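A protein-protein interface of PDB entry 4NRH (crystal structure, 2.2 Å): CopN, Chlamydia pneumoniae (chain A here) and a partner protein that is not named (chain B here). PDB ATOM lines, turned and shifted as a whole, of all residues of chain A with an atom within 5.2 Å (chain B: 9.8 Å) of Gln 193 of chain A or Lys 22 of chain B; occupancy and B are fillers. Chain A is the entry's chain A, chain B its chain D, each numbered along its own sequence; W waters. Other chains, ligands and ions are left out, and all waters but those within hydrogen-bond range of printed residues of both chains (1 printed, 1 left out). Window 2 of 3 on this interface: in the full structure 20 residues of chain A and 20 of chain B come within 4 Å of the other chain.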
ATOM      1  N   ALA A 156      -6.127  31.611 -14.217  1.00  0.00           N
ATOM      2  CA  ALA A 156      -5.326  30.607 -13.523  1.00  0.00           C
ATOM      3  C   ALA A 156      -6.213  29.598 -12.799  1.00  0.00           C
ATOM      4  O   ALA A 156      -6.023  28.388 -12.927  1.00  0.00           O
ATOM      5  CB  ALA A 156      -4.372  31.274 -12.547  1.00  0.00           C
ATOM      6  N   SER A 159      -8.159  27.594 -15.365  1.00  0.00           N
ATOM      7  CA  SER A 159      -7.296  26.584 -15.970  1.00  0.00           C
ATOM      8  C   SER A 159      -7.155  25.370 -15.056  1.00  0.00           C
ATOM      9  O   SER A 159      -7.113  24.232 -15.523  1.00  0.00           O
ATOM     10  CB  SER A 159      -5.919  27.169 -16.284  1.00  0.00           C
ATOM     11  OG  SER A 159      -5.203  27.453 -15.095  1.00  0.00           O
ATOM     12  N   SER A 160      -7.078  25.621 -13.753  1.00  0.00           N
ATOM     13  CA  SER A 160      -6.979  24.548 -12.769  1.00  0.00           C
ATOM     14  C   SER A 160      -8.267  23.730 -12.715  1.00  0.00           C
ATOM     15  O   SER A 160      -8.229  22.511 -12.548  1.00  0.00           O
ATOM     16  CB  SER A 160      -6.656  25.114 -11.385  1.00  0.00           C
ATOM     17  OG  SER A 160      -5.377  25.722 -11.371  1.00  0.00           O
ATOM     18  N   MET A 163      -8.212  21.396 -15.668  1.00  0.00           N
ATOM     19  CA  MET A 163      -7.305  20.282 -15.408  1.00  0.00           C
ATOM     20  C   MET A 163      -7.937  19.268 -14.461  1.00  0.00           C
ATOM     21  O   MET A 163      -7.804  18.059 -14.652  1.00  0.00           O
ATOM     22  CB  MET A 163      -5.985  20.785 -14.826  1.00  0.00           C
ATOM     23  CG  MET A 163      -5.147  21.598 -15.795  1.00  0.00           C
ATOM     24  SD  MET A 163      -4.483  20.594 -17.138  1.00  0.00           S
ATOM     25  CE  MET A 163      -3.415  19.479 -16.229  1.00  0.00           C
ATOM     26  N   THR A 189      -3.498  22.438 -22.098  1.00  0.00           N
ATOM     27  CA  THR A 189      -3.927  23.264 -20.977  1.00  0.00           C
ATOM     28  C   THR A 189      -2.743  23.582 -20.064  1.00  0.00           C
ATOM     29  O   THR A 189      -2.657  24.676 -19.503  1.00  0.00           O
ATOM     30  CB  THR A 189      -5.045  22.580 -20.165  1.00  0.00           C
ATOM     31  OG1 THR A 189      -6.147  22.276 -21.029  1.00  0.00           O
ATOM     32  CG2 THR A 189      -5.528  23.485 -19.040  1.00  0.00           C
ATOM     33  N   ARG A 190      -1.829  22.627 -19.922  1.00  0.00           N
ATOM     34  CA  ARG A 190      -0.586  22.866 -19.195  1.00  0.00           C
ATOM     35  C   ARG A 190       0.240  23.944 -19.890  1.00  0.00           C
ATOM     36  O   ARG A 190       0.857  24.785 -19.238  1.00  0.00           O
ATOM     37  CB  ARG A 190       0.227  21.576 -19.052  1.00  0.00           C
ATOM     38  CG  ARG A 190      -0.350  20.589 -18.050  1.00  0.00           C
ATOM     39  CD  ARG A 190       0.550  19.374 -17.889  1.00  0.00           C
ATOM     40  NE  ARG A 190       0.105  18.508 -16.801  1.00  0.00           N
ATOM     41  CZ  ARG A 190      -0.454  17.315 -16.977  1.00  0.00           C
ATOM     42  NH1 ARG A 190      -0.637  16.839 -18.201  1.00  0.00           N
ATOM     43  NH2 ARG A 190      -0.830  16.598 -15.926  1.00  0.00           N
ATOM     44  N   ASN A 191       0.255  23.907 -21.220  1.00  0.00           N
ATOM     45  CA  ASN A 191       0.925  24.934 -22.004  1.00  0.00           C
ATOM     46  C   ASN A 191       0.261  26.293 -21.817  1.00  0.00           C
ATOM     47  O   ASN A 191       0.930  27.324 -21.804  1.00  0.00           O
ATOM     48  CB  ASN A 191       0.942  24.556 -23.487  1.00  0.00           C
ATOM     49  CG  ASN A 191       1.812  23.347 -23.769  1.00  0.00           C
ATOM     50  OD1 ASN A 191       2.598  22.922 -22.922  1.00  0.00           O
ATOM     51  ND2 ASN A 191       1.672  22.785 -24.964  1.00  0.00           N
ATOM     52  N   LEU A 192      -1.063  26.284 -21.683  1.00  0.00           N
ATOM     53  CA  LEU A 192      -1.818  27.501 -21.401  1.00  0.00           C
ATOM     54  C   LEU A 192      -1.393  28.106 -20.068  1.00  0.00           C
ATOM     55  O   LEU A 192      -1.192  29.316 -19.962  1.00  0.00           O
ATOM     56  CB  LEU A 192      -3.322  27.219 -21.398  1.00  0.00           C
ATOM     57  CG  LEU A 192      -4.214  28.387 -20.969  1.00  0.00           C
ATOM     58  CD1 LEU A 192      -4.001  29.587 -21.882  1.00  0.00           C
ATOM     59  CD2 LEU A 192      -5.677  27.976 -20.947  1.00  0.00           C
ATOM     60  N   GLN A 193      -1.271  27.257 -19.052  1.00  0.00           N
ATOM     61  CA  GLN A 193      -0.878  27.704 -17.720  1.00  0.00           C
ATOM     62  C   GLN A 193       0.521  28.314 -17.731  1.00  0.00           C
ATOM     63  O   GLN A 193       0.807  29.242 -16.978  1.00  0.00           O
ATOM     64  CB  GLN A 193      -0.938  26.543 -16.725  1.00  0.00           C
ATOM     65  CG  GLN A 193      -2.342  26.016 -16.474  1.00  0.00           C
ATOM     66  CD  GLN A 193      -2.391  25.009 -15.341  1.00  0.00           C
ATOM     67  OE1 GLN A 193      -1.544  24.120 -15.247  1.00  0.00           O
ATOM     68  NE2 GLN A 193      -3.385  25.146 -14.471  1.00  0.00           N
ATOM     69  N   ALA A 194       1.386  27.785 -18.592  1.00  0.00           N
ATOM     70  CA  ALA A 194       2.732  28.324 -18.749  1.00  0.00           C
ATOM     71  C   ALA A 194       2.674  29.711 -19.381  1.00  0.00           C
ATOM     72  O   ALA A 194       3.344  30.642 -18.931  1.00  0.00           O
ATOM     73  CB  ALA A 194       3.589  27.389 -19.589  1.00  0.00           C
ATOM     74  N   VAL A 195       1.869  29.835 -20.432  1.00  0.00           N
ATOM     75  CA  VAL A 195       1.654  31.109 -21.109  1.00  0.00           C
ATOM     76  C   VAL A 195       1.094  32.165 -20.154  1.00  0.00           C
ATOM     77  O   VAL A 195       1.503  33.327 -20.188  1.00  0.00           O
ATOM     78  CB  VAL A 195       0.701  30.938 -22.315  1.00  0.00           C
ATOM     79  CG1 VAL A 195       0.227  32.287 -22.832  1.00  0.00           C
ATOM     80  CG2 VAL A 195       1.390  30.154 -23.422  1.00  0.00           C
ATOM     81  N   LEU A 196       0.175  31.746 -19.288  1.00  0.00           N
ATOM     82  CA  LEU A 196      -0.452  32.648 -18.324  1.00  0.00           C
ATOM     83  C   LEU A 196       0.545  33.283 -17.356  1.00  0.00           C
ATOM     84  O   LEU A 196       0.336  34.404 -16.894  1.00  0.00           O
ATOM     85  CB  LEU A 196      -1.534  31.910 -17.531  1.00  0.00           C
ATOM     86  CG  LEU A 196      -2.842  31.616 -18.269  1.00  0.00           C
ATOM     87  CD1 LEU A 196      -3.770  30.786 -17.400  1.00  0.00           C
ATOM     88  CD2 LEU A 196      -3.513  32.911 -18.693  1.00  0.00           C
ATOM     89  N   THR A 197       1.617  32.562 -17.040  1.00  0.00           N
ATOM     90  CA  THR A 197       2.640  33.078 -16.134  1.00  0.00           C
ATOM     91  C   THR A 197       3.281  34.349 -16.684  1.00  0.00           C
ATOM     92  O   THR A 197       3.640  35.249 -15.925  1.00  0.00           O
ATOM     93  CB  THR A 197       3.743  32.037 -15.866  1.00  0.00           C
ATOM     94  OG1 THR A 197       4.448  31.759 -17.082  1.00  0.00           O
ATOM     95  CG2 THR A 197       3.142  30.747 -15.325  1.00  0.00           C
ATOM     96  N   ASP A 200       0.776  37.177 -16.313  1.00  0.00           N
ATOM     97  CA  ASP A 200       0.774  37.502 -14.891  1.00  0.00           C
ATOM     98  C   ASP A 200       2.001  38.330 -14.527  1.00  0.00           C
ATOM     99  O   ASP A 200       1.908  39.300 -13.773  1.00  0.00           O
ATOM    100  CB  ASP A 200       0.726  36.227 -14.046  1.00  0.00           C
ATOM    101  CG  ASP A 200       0.824  36.509 -12.557  1.00  0.00           C
ATOM    102  OD1 ASP A 200       1.958  36.633 -12.044  1.00  0.00           O
ATOM    103  OD2 ASP A 200      -0.233  36.607 -11.897  1.00  0.00           O
ATOM    104  N   LYS B  16       6.762  19.683  -4.462  1.00  0.00           N
ATOM    105  CA  LYS B  16       6.976  20.915  -3.709  1.00  0.00           C
ATOM    106  C   LYS B  16       6.951  22.134  -4.629  1.00  0.00           C
ATOM    107  O   LYS B  16       6.291  23.133  -4.338  1.00  0.00           O
ATOM    108  CB  LYS B  16       8.303  20.843  -2.948  1.00  0.00           C
ATOM    109  CG  LYS B  16       8.586  22.024  -2.036  1.00  0.00           C
ATOM    110  CD  LYS B  16       9.739  21.707  -1.093  1.00  0.00           C
ATOM    111  CE  LYS B  16      10.155  22.920  -0.278  1.00  0.00           C
ATOM    112  NZ  LYS B  16      10.582  24.057  -1.140  1.00  0.00           N
ATOM    113  N   ILE B  17       7.675  22.041  -5.741  1.00  0.00           N
ATOM    114  CA  ILE B  17       7.728  23.119  -6.725  1.00  0.00           C
ATOM    115  C   ILE B  17       6.382  23.328  -7.418  1.00  0.00           C
ATOM    116  O   ILE B  17       5.908  24.457  -7.545  1.00  0.00           O
ATOM    117  CB  ILE B  17       8.806  22.846  -7.795  1.00  0.00           C
ATOM    118  CG1 ILE B  17      10.199  22.839  -7.163  1.00  0.00           C
ATOM    119  CG2 ILE B  17       8.734  23.884  -8.903  1.00  0.00           C
ATOM    120  CD1 ILE B  17      11.279  22.304  -8.079  1.00  0.00           C
ATOM    121  N   ALA B  18       5.772  22.231  -7.862  1.00  0.00           N
ATOM    122  CA  ALA B  18       4.490  22.282  -8.560  1.00  0.00           C
ATOM    123  C   ALA B  18       3.405  22.909  -7.695  1.00  0.00           C
ATOM    124  O   ALA B  18       2.603  23.712  -8.175  1.00  0.00           O
ATOM    125  CB  ALA B  18       4.071  20.888  -9.000  1.00  0.00           C
ATOM    126  N   ALA B  19       3.378  22.525  -6.423  1.00  0.00           N
ATOM    127  CA  ALA B  19       2.391  23.042  -5.484  1.00  0.00           C
ATOM    128  C   ALA B  19       2.454  24.563  -5.374  1.00  0.00           C
ATOM    129  O   ALA B  19       1.430  25.236  -5.452  1.00  0.00           O
ATOM    130  CB  ALA B  19       2.580  22.407  -4.114  1.00  0.00           C
ATOM    131  N   SER B  20       3.662  25.100  -5.240  1.00  0.00           N
ATOM    132  CA  SER B  20       3.843  26.531  -5.007  1.00  0.00           C
ATOM    133  C   SER B  20       3.713  27.366  -6.279  1.00  0.00           C
ATOM    134  O   SER B  20       3.907  28.580  -6.253  1.00  0.00           O
ATOM    135  CB  SER B  20       5.209  26.789  -4.365  1.00  0.00           C
ATOM    136  OG  SER B  20       6.249  26.209  -5.130  1.00  0.00           O
ATOM    137  N   SER B  21       3.389  26.714  -7.390  1.00  0.00           N
ATOM    138  CA  SER B  21       3.141  27.422  -8.638  1.00  0.00           C
ATOM    139  C   SER B  21       1.648  27.447  -8.952  1.00  0.00           C
ATOM    140  O   SER B  21       0.857  26.775  -8.291  1.00  0.00           O
ATOM    141  CB  SER B  21       3.915  26.777  -9.789  1.00  0.00           C
ATOM    142  OG  SER B  21       3.185  25.706 -10.359  1.00  0.00           O
ATOM    143  N   LYS B  22       1.269  28.221  -9.963  1.00  0.00           N
ATOM    144  CA  LYS B  22      -0.114  28.257 -10.419  1.00  0.00           C
ATOM    145  C   LYS B  22      -0.310  27.253 -11.544  1.00  0.00           C
ATOM    146  O   LYS B  22      -1.307  27.292 -12.265  1.00  0.00           O
ATOM    147  CB  LYS B  22      -0.500  29.659 -10.893  1.00  0.00           C
ATOM    148  CG  LYS B  22      -0.513  30.719  -9.806  1.00  0.00           C
ATOM    149  CD  LYS B  22      -0.979  32.055 -10.366  1.00  0.00           C
ATOM    150  CE  LYS B  22      -0.915  33.151  -9.320  1.00  0.00           C
ATOM    151  NZ  LYS B  22      -1.766  32.830  -8.145  1.00  0.00           N
ATOM    152  N   GLU B  23       0.656  26.353 -11.688  1.00  0.00           N
ATOM    153  CA  GLU B  23       0.633  25.363 -12.754  1.00  0.00           C
ATOM    154  C   GLU B  23       0.549  23.950 -12.194  1.00  0.00           C
ATOM    155  O   GLU B  23       1.127  23.650 -11.148  1.00  0.00           O
ATOM    156  CB  GLU B  23       1.880  25.499 -13.628  1.00  0.00           C
ATOM    157  CG  GLU B  23       2.075  26.880 -14.225  1.00  0.00           C
ATOM    158  CD  GLU B  23       3.489  27.097 -14.729  1.00  0.00           C
ATOM    159  OE1 GLU B  23       4.233  27.879 -14.099  1.00  0.00           O
ATOM    160  OE2 GLU B  23       3.854  26.491 -15.757  1.00  0.00           O
ATOM    161  N   ASP B  24      -0.179  23.089 -12.896  1.00  0.00           N
ATOM    162  CA  ASP B  24      -0.250  21.675 -12.553  1.00  0.00           C
ATOM    163  C   ASP B  24       1.130  21.034 -12.644  1.00  0.00           C
ATOM    164  O   ASP B  24       1.529  20.258 -11.775  1.00  0.00           O
ATOM    165  CB  ASP B  24      -1.231  20.945 -13.473  1.00  0.00           C
ATOM    166  CG  ASP B  24      -1.229  19.444 -13.256  1.00  0.00           C
ATOM    167  OD1 ASP B  24      -1.901  18.978 -12.313  1.00  0.00           O
ATOM    168  OD2 ASP B  24      -0.556  18.730 -14.030  1.00  0.00           O
ATOM    169  N   PHE B  25       1.851  21.367 -13.709  1.00  0.00           N
ATOM    170  CA  PHE B  25       3.152  20.772 -13.982  1.00  0.00           C
ATOM    171  C   PHE B  25       4.053  21.788 -14.677  1.00  0.00           C
ATOM    172  O   PHE B  25       4.082  21.863 -15.906  1.00  0.00           O
ATOM    173  CB  PHE B  25       2.985  19.517 -14.843  1.00  0.00           C
ATOM    174  CG  PHE B  25       4.247  18.728 -15.029  1.00  0.00           C
ATOM    175  CD1 PHE B  25       4.799  18.019 -13.975  1.00  0.00           C
ATOM    176  CD2 PHE B  25       4.874  18.682 -16.264  1.00  0.00           C
ATOM    177  CE1 PHE B  25       5.959  17.284 -14.147  1.00  0.00           C
ATOM    178  CE2 PHE B  25       6.033  17.951 -16.441  1.00  0.00           C
ATOM    179  CZ  PHE B  25       6.576  17.251 -15.382  1.00  0.00           C
ATOM    180  N   PRO B  26       4.792  22.582 -13.886  1.00  0.00           N
ATOM    181  CA  PRO B  26       5.569  23.712 -14.409  1.00  0.00           C
ATOM    182  C   PRO B  26       6.921  23.298 -14.983  1.00  0.00           C
ATOM    183  O   PRO B  26       7.932  23.944 -14.709  1.00  0.00           O
ATOM    184  CB  PRO B  26       5.755  24.597 -13.176  1.00  0.00           C
ATOM    185  CG  PRO B  26       5.786  23.630 -12.041  1.00  0.00           C
ATOM    186  CD  PRO B  26       4.857  22.501 -12.416  1.00  0.00           C
ATOM    187  N   PHE B  27       6.927  22.234 -15.777  1.00  0.00           N
ATOM    188  CA  PHE B  27       8.154  21.705 -16.358  1.00  0.00           C
ATOM    189  C   PHE B  27       7.901  21.253 -17.792  1.00  0.00           C
ATOM    190  O   PHE B  27       6.752  21.025 -18.175  1.00  0.00           O
ATOM    191  CB  PHE B  27       8.686  20.533 -15.529  1.00  0.00           C
ATOM    192  CG  PHE B  27       8.792  20.824 -14.060  1.00  0.00           C
ATOM    193  CD1 PHE B  27       9.807  21.629 -13.572  1.00  0.00           C
ATOM    194  CD2 PHE B  27       7.886  20.279 -13.166  1.00  0.00           C
ATOM    195  CE1 PHE B  27       9.911  21.891 -12.219  1.00  0.00           C
ATOM    196  CE2 PHE B  27       7.985  20.537 -11.812  1.00  0.00           C
ATOM    197  CZ  PHE B  27       8.999  21.344 -11.338  1.00  0.00           C
ATOM    198  N   PHE B  53      14.187  27.841  -8.308  1.00  0.00           N
ATOM    199  CA  PHE B  53      13.262  27.065  -7.485  1.00  0.00           C
ATOM    200  C   PHE B  53      13.758  26.932  -6.048  1.00  0.00           C
ATOM    201  O   PHE B  53      13.164  26.210  -5.245  1.00  0.00           O
ATOM    202  CB  PHE B  53      13.038  25.677  -8.089  1.00  0.00           C
ATOM    203  CG  PHE B  53      12.293  25.695  -9.394  1.00  0.00           C
ATOM    204  CD1 PHE B  53      11.176  26.497  -9.557  1.00  0.00           C
ATOM    205  CD2 PHE B  53      12.712  24.912 -10.458  1.00  0.00           C
ATOM    206  CE1 PHE B  53      10.488  26.517 -10.756  1.00  0.00           C
ATOM    207  CE2 PHE B  53      12.029  24.928 -11.661  1.00  0.00           C
ATOM    208  CZ  PHE B  53      10.915  25.732 -11.809  1.00  0.00           C
HETATM  209  O   HOH W   1       1.131  22.833 -15.680  1.00  0.00           O
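OD2 of Asp 24 of chain B lies within salt-bridge range of NE of Arg 190 of chain A (2.9 Å). OE1 of Gln 193 of chain A is in hydrogen-bond range of N of Asp 24 of chain B.
OG1 of Thr 197 of chain A sits at hydrogen-bond distance from O of Ala 194 of chain A (2.4 Å). OG of Ser 159 of chain A is in hydrogen-bond range of NE2 of Gln 193 of chain A. The side-chain hydroxyl (OG) of Ser 21 of chain B lies within hydrogen-bond range of the backbone NH (N) of Glu 23 of chain B, at 2.9 Å.
Asp 24 of chain B touches Met 163 of chain A. NE of Arg 190 of chain A touches CB of Phe 25 of chain B, 3.6 Å away. Gln 193 of chain A touches Lys 22 of chain B (NE2 to O, 3.7 Å). Glu 23 of chain B touches Gln 193 of chain A. Glu 23 of chain B touches Ala 194 of chain A (OE2 to CA, 3.7 Å). Thr 197 of chain A touches Glu 23 of chain B.
Of the printed residues of chain B, Met 163 of chain A touches Asp 24 (3.7 Å). Of the printed residues of chain B, Arg 190 of chain A touches Asp 24 and Phe 25. Asn 191 of chain A touches none of the printed residues of chain B. No residue of chain B comes within 4 Å of Leu 192 of chain A. Of the printed residues of chain B, Gln 193 of chain A touches Lys 22 (3.7 Å), Glu 23 (3.5 Å) and Asp 24 (2.9 Å). Of the printed residues of chain B, Ala 194 of chain A touches Glu 23 (3.7 Å). Of the printed residues of chain B, Thr 197 of chain A touches Glu 23. Ser 20 of chain B touches none of the printed residues of chain A. Of the printed residues of chain A, Lys 22 of chain B touches Gln 193. Of the printed residues of chain A, Glu 23 of chain B touches Gln 193 (3.5 Å), Ala 194 (3.7 Å) and Thr 197 (3.3 Å). Of the printed residues of chain A, Phe 25 of chain B touches Arg 190. The nearest residue of chain A that does not touch Lys 22 of chain B is Ala 156 of chain A (4.1 Å). The nearest printed residue of chain A that does not touch Glu 23 of chain B is Arg 190 of chain A (4.9 Å).
Printed residues of chain A that touch a printed residue of chain B: Met 163, Arg 190, Gln 193, Ala 194 and Thr 197. Hydrophobic or aromatic side chains of chain A within 4 Å of the printed part of chain B: Met 163 and Ala 194. Among the printed residues, 8 pairs touch across the chains. Among the printed residues, Asp or Glu carboxylates within 4 Å of a Lys or Arg side-chain nitrogen of the other chain: Arg 190 of chain A with Asp 24 of chain B.
Water W1 lies within hydrogen-bond range of the backbone NH (N) of Phe 25 of chain B (2.6 Å), the side-chain amide oxygen (OE1) of Gln 193 of chain A (3.0 Å) and the backbone NH (N) of Asp 24 of chain B (3.1 Å).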
